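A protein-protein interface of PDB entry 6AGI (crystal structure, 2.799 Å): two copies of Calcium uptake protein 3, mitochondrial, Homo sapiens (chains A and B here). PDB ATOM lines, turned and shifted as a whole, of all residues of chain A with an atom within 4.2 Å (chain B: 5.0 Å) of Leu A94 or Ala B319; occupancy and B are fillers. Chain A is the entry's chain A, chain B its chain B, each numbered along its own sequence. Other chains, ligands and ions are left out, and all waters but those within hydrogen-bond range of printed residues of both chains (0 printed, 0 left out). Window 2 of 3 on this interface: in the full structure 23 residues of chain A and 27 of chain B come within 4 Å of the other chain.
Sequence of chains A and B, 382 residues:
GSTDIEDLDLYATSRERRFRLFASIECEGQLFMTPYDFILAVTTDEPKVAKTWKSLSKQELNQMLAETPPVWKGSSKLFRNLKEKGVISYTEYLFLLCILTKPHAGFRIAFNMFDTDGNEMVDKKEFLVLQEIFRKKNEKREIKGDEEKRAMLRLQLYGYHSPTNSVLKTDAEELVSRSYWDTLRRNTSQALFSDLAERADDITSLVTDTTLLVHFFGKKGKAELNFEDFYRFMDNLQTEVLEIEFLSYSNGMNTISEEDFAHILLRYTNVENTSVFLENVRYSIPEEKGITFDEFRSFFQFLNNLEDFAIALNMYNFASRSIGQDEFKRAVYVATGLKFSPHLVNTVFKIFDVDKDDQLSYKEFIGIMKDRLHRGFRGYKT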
ATOM      1  N   TYR A  90      -5.354 -24.590 -13.931  1.00  0.00           N
ATOM      2  CA  TYR A  90      -6.008 -25.180 -15.092  1.00  0.00           C
ATOM      3  C   TYR A  90      -4.986 -25.571 -16.150  1.00  0.00           C
ATOM      4  O   TYR A  90      -5.012 -26.694 -16.682  1.00  0.00           O
ATOM      5  CB  TYR A  90      -7.026 -24.221 -15.699  1.00  0.00           C
ATOM      6  CG  TYR A  90      -7.634 -24.775 -16.976  1.00  0.00           C
ATOM      7  CD1 TYR A  90      -8.374 -25.956 -16.957  1.00  0.00           C
ATOM      8  CD2 TYR A  90      -7.418 -24.155 -18.206  1.00  0.00           C
ATOM      9  CE1 TYR A  90      -8.924 -26.473 -18.120  1.00  0.00           C
ATOM     10  CE2 TYR A  90      -7.957 -24.663 -19.373  1.00  0.00           C
ATOM     11  CZ  TYR A  90      -8.707 -25.818 -19.330  1.00  0.00           C
ATOM     12  OH  TYR A  90      -9.229 -26.308 -20.511  1.00  0.00           O
ATOM     13  N   THR A  91      -4.101 -24.628 -16.504  1.00  0.00           N
ATOM     14  CA  THR A  91      -3.020 -24.930 -17.441  1.00  0.00           C
ATOM     15  C   THR A  91      -2.212 -26.140 -17.012  1.00  0.00           C
ATOM     16  O   THR A  91      -1.927 -27.015 -17.831  1.00  0.00           O
ATOM     17  CB  THR A  91      -2.130 -23.710 -17.640  1.00  0.00           C
ATOM     18  OG1 THR A  91      -2.927 -22.582 -18.003  1.00  0.00           O
ATOM     19  CG2 THR A  91      -1.006 -24.011 -18.667  1.00  0.00           C
ATOM     20  N   GLU A  92      -1.805 -26.191 -15.749  1.00  0.00           N
ATOM     21  CA  GLU A  92      -1.006 -27.322 -15.308  1.00  0.00           C
ATOM     22  C   GLU A  92      -1.802 -28.619 -15.414  1.00  0.00           C
ATOM     23  O   GLU A  92      -1.260 -29.660 -15.806  1.00  0.00           O
ATOM     24  CB  GLU A  92      -0.504 -27.086 -13.891  1.00  0.00           C
ATOM     25  CG  GLU A  92       0.547 -26.015 -13.824  1.00  0.00           C
ATOM     26  CD  GLU A  92       0.715 -25.422 -12.439  1.00  0.00           C
ATOM     27  OE1 GLU A  92      -0.208 -25.540 -11.595  1.00  0.00           O
ATOM     28  OE2 GLU A  92       1.788 -24.825 -12.205  1.00  0.00           O
ATOM     29  N   TYR A  93      -3.094 -28.566 -15.084  1.00  0.00           N
ATOM     30  CA  TYR A  93      -3.992 -29.688 -15.340  1.00  0.00           C
ATOM     31  C   TYR A  93      -3.875 -30.178 -16.786  1.00  0.00           C
ATOM     32  O   TYR A  93      -3.680 -31.385 -17.039  1.00  0.00           O
ATOM     33  CB  TYR A  93      -5.425 -29.265 -14.994  1.00  0.00           C
ATOM     34  CG  TYR A  93      -6.519 -30.240 -15.376  1.00  0.00           C
ATOM     35  CD1 TYR A  93      -6.364 -31.624 -15.236  1.00  0.00           C
ATOM     36  CD2 TYR A  93      -7.718 -29.764 -15.896  1.00  0.00           C
ATOM     37  CE1 TYR A  93      -7.387 -32.505 -15.606  1.00  0.00           C
ATOM     38  CE2 TYR A  93      -8.736 -30.633 -16.274  1.00  0.00           C
ATOM     39  CZ  TYR A  93      -8.568 -31.995 -16.132  1.00  0.00           C
ATOM     40  OH  TYR A  93      -9.586 -32.841 -16.495  1.00  0.00           O
ATOM     41  N   LEU A  94      -4.022 -29.256 -17.749  1.00  0.00           N
ATOM     42  CA  LEU A  94      -3.872 -29.621 -19.156  1.00  0.00           C
ATOM     43  C   LEU A  94      -2.521 -30.279 -19.401  1.00  0.00           C
ATOM     44  O   LEU A  94      -2.446 -31.399 -19.940  1.00  0.00           O
ATOM     45  CB  LEU A  94      -4.033 -28.383 -20.048  1.00  0.00           C
ATOM     46  CG  LEU A  94      -5.444 -27.783 -20.126  1.00  0.00           C
ATOM     47  CD1 LEU A  94      -5.643 -27.060 -21.441  1.00  0.00           C
ATOM     48  CD2 LEU A  94      -6.557 -28.820 -19.910  1.00  0.00           C
ATOM     49  N   PHE A  95      -1.451 -29.606 -18.955  1.00  0.00           N
ATOM     50  CA  PHE A  95      -0.100 -30.138 -19.056  1.00  0.00           C
ATOM     51  C   PHE A  95      -0.059 -31.612 -18.649  1.00  0.00           C
ATOM     52  O   PHE A  95       0.362 -32.457 -19.435  1.00  0.00           O
ATOM     53  CB  PHE A  95       0.836 -29.271 -18.213  1.00  0.00           C
ATOM     54  CG  PHE A  95       2.283 -29.688 -18.245  1.00  0.00           C
ATOM     55  CD1 PHE A  95       2.968 -29.857 -19.440  1.00  0.00           C
ATOM     56  CD2 PHE A  95       2.968 -29.879 -17.057  1.00  0.00           C
ATOM     57  CE1 PHE A  95       4.306 -30.237 -19.444  1.00  0.00           C
ATOM     58  CE2 PHE A  95       4.298 -30.260 -17.046  1.00  0.00           C
ATOM     59  CZ  PHE A  95       4.973 -30.438 -18.245  1.00  0.00           C
ATOM     60  N   LEU A  96      -0.554 -31.935 -17.447  1.00  0.00           N
ATOM     61  CA  LEU A  96      -0.478 -33.295 -16.906  1.00  0.00           C
ATOM     62  C   LEU A  96      -1.295 -34.317 -17.713  1.00  0.00           C
ATOM     63  O   LEU A  96      -0.863 -35.480 -17.867  1.00  0.00           O
ATOM     64  CB  LEU A  96      -0.912 -33.278 -15.438  1.00  0.00           C
ATOM     65  CG  LEU A  96      -0.085 -32.375 -14.514  1.00  0.00           C
ATOM     66  CD1 LEU A  96      -0.755 -32.228 -13.162  1.00  0.00           C
ATOM     67  CD2 LEU A  96       1.342 -32.888 -14.337  1.00  0.00           C
ATOM     68  N   LEU A  97      -2.505 -33.936 -18.159  1.00  0.00           N
ATOM     69  CA  LEU A  97      -3.267 -34.774 -19.100  1.00  0.00           C
ATOM     70  C   LEU A  97      -2.407 -35.182 -20.282  1.00  0.00           C
ATOM     71  O   LEU A  97      -2.218 -36.373 -20.601  1.00  0.00           O
ATOM     72  CB  LEU A  97      -4.436 -33.974 -19.638  1.00  0.00           C
ATOM     73  CG  LEU A  97      -5.657 -33.537 -18.815  1.00  0.00           C
ATOM     74  CD1 LEU A  97      -6.585 -32.779 -19.746  1.00  0.00           C
ATOM     75  CD2 LEU A  97      -6.404 -34.694 -18.126  1.00  0.00           C
ATOM     76  N   CYS A  98      -1.857 -34.155 -20.920  1.00  0.00           N
ATOM     77  CA  CYS A  98      -1.012 -34.307 -22.098  1.00  0.00           C
ATOM     78  C   CYS A  98       0.172 -35.218 -21.794  1.00  0.00           C
ATOM     79  O   CYS A  98       0.490 -36.122 -22.578  1.00  0.00           O
ATOM     80  CB  CYS A  98      -0.584 -32.892 -22.543  1.00  0.00           C
ATOM     81  SG  CYS A  98       0.681 -32.760 -23.746  1.00  0.00           S
ATOM     82  N   MET B 315      -0.671 -29.985 -26.689  1.00  0.00           N
ATOM     83  CA  MET B 315      -1.079 -29.039 -25.658  1.00  0.00           C
ATOM     84  C   MET B 315      -2.075 -28.037 -26.224  1.00  0.00           C
ATOM     85  O   MET B 315      -3.057 -27.686 -25.557  1.00  0.00           O
ATOM     86  CB  MET B 315       0.156 -28.304 -25.124  1.00  0.00           C
ATOM     87  CG  MET B 315       0.584 -28.616 -23.683  1.00  0.00           C
ATOM     88  SD  MET B 315      -0.754 -28.553 -22.492  1.00  0.00           S
ATOM     89  CE  MET B 315      -0.645 -26.888 -21.876  1.00  0.00           C
ATOM     90  N   TYR B 316      -1.879 -27.638 -27.489  1.00  0.00           N
ATOM     91  CA  TYR B 316      -2.869 -26.819 -28.182  1.00  0.00           C
ATOM     92  C   TYR B 316      -4.198 -27.530 -28.328  1.00  0.00           C
ATOM     93  O   TYR B 316      -5.257 -26.911 -28.146  1.00  0.00           O
ATOM     94  CB  TYR B 316      -2.368 -26.398 -29.569  1.00  0.00           C
ATOM     95  CG  TYR B 316      -1.295 -25.345 -29.549  1.00  0.00           C
ATOM     96  CD1 TYR B 316       0.010 -25.636 -29.162  1.00  0.00           C
ATOM     97  CD2 TYR B 316      -1.615 -24.028 -29.842  1.00  0.00           C
ATOM     98  CE1 TYR B 316       0.981 -24.649 -29.127  1.00  0.00           C
ATOM     99  CE2 TYR B 316      -0.658 -23.038 -29.803  1.00  0.00           C
ATOM    100  CZ  TYR B 316       0.633 -23.346 -29.446  1.00  0.00           C
ATOM    101  OH  TYR B 316       1.575 -22.339 -29.413  1.00  0.00           O
ATOM    102  N   ASN B 317      -4.180 -28.828 -28.664  1.00  0.00           N
ATOM    103  CA  ASN B 317      -5.483 -29.437 -28.923  1.00  0.00           C
ATOM    104  C   ASN B 317      -6.239 -29.748 -27.627  1.00  0.00           C
ATOM    105  O   ASN B 317      -7.482 -29.673 -27.601  1.00  0.00           O
ATOM    106  CB  ASN B 317      -5.311 -30.685 -29.786  1.00  0.00           C
ATOM    107  CG  ASN B 317      -6.575 -31.534 -29.873  1.00  0.00           C
ATOM    108  OD1 ASN B 317      -7.694 -31.003 -29.795  1.00  0.00           O
ATOM    109  ND2 ASN B 317      -6.411 -32.844 -30.054  1.00  0.00           N
ATOM    110  N   PHE B 318      -5.531 -29.990 -26.514  1.00  0.00           N
ATOM    111  CA  PHE B 318      -6.243 -30.137 -25.244  1.00  0.00           C
ATOM    112  C   PHE B 318      -6.954 -28.849 -24.852  1.00  0.00           C
ATOM    113  O   PHE B 318      -7.966 -28.894 -24.139  1.00  0.00           O
ATOM    114  CB  PHE B 318      -5.303 -30.611 -24.132  1.00  0.00           C
ATOM    115  CG  PHE B 318      -5.228 -32.112 -24.012  1.00  0.00           C
ATOM    116  CD1 PHE B 318      -6.232 -32.827 -23.380  1.00  0.00           C
ATOM    117  CD2 PHE B 318      -4.175 -32.813 -24.572  1.00  0.00           C
ATOM    118  CE1 PHE B 318      -6.176 -34.219 -23.290  1.00  0.00           C
ATOM    119  CE2 PHE B 318      -4.112 -34.197 -24.491  1.00  0.00           C
ATOM    120  CZ  PHE B 318      -5.110 -34.899 -23.847  1.00  0.00           C
ATOM    121  N   ALA B 319      -6.451 -27.701 -25.301  1.00  0.00           N
ATOM    122  CA  ALA B 319      -7.029 -26.415 -24.945  1.00  0.00           C
ATOM    123  C   ALA B 319      -7.985 -25.864 -25.996  1.00  0.00           C
ATOM    124  O   ALA B 319      -8.530 -24.775 -25.797  1.00  0.00           O
ATOM    125  CB  ALA B 319      -5.920 -25.390 -24.688  1.00  0.00           C
ATOM    126  N   SER B 320      -8.203 -26.574 -27.099  1.00  0.00           N
ATOM    127  CA  SER B 320      -8.992 -26.051 -28.217  1.00  0.00           C
ATOM    128  C   SER B 320      -8.528 -24.643 -28.597  1.00  0.00           C
ATOM    129  O   SER B 320      -9.272 -23.661 -28.533  1.00  0.00           O
ATOM    130  CB  SER B 320     -10.492 -26.075 -27.913  1.00  0.00           C
ATOM    131  OG  SER B 320     -10.982 -27.401 -27.885  1.00  0.00           O
ATOM    132  N   ARG B 321      -7.267 -24.560 -29.000  1.00  0.00           N
ATOM    133  CA  ARG B 321      -6.666 -23.300 -29.392  1.00  0.00           C
ATOM    134  C   ARG B 321      -6.009 -23.494 -30.752  1.00  0.00           C
ATOM    135  O   ARG B 321      -5.732 -24.623 -31.181  1.00  0.00           O
ATOM    136  CB  ARG B 321      -5.647 -22.810 -28.355  1.00  0.00           C
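The side-chain sulfur of Met B315 lies within hydrogen-bond range of the backbone NH of Phe A95 (3.8 Å).
No position is printed for both chains.
Of the printed residues of chain A, Ala B319 touches Leu A94 (3.7 Å).
Of the printed residues of chain A, Met B315 touches Leu A94 (3.96 Å) and Phe A95 (3.8 Å).
Of the printed residues of chain A, Phe B318 touches Leu A97 (3.7 Å) and Cys A98 (3.9 Å).
The nearest printed residue of chain A that does not touch Phe B318 is Leu A94 (4.005 Å).
Among the printed residues, pairs that only touch across the chains: Leu A94 with Met B315, Leu A94 with Ala B319, Leu A97 with Phe B318 and Cys A98 with Phe B318.
Hydrophobic or aromatic side chains of chain A within 4 Å of the printed part of chain B: Leu A94 and Leu A97.
Along chain A the printed residues that touch a printed residue of chain B span positions 94 to 98.
Of the 7 printed residues of chain B, 3 touch a printed residue of chain A.
Hydrophobic or aromatic side chains of chain B that line the printed part of chain A: Met B315, Phe B318 and Ala B319.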
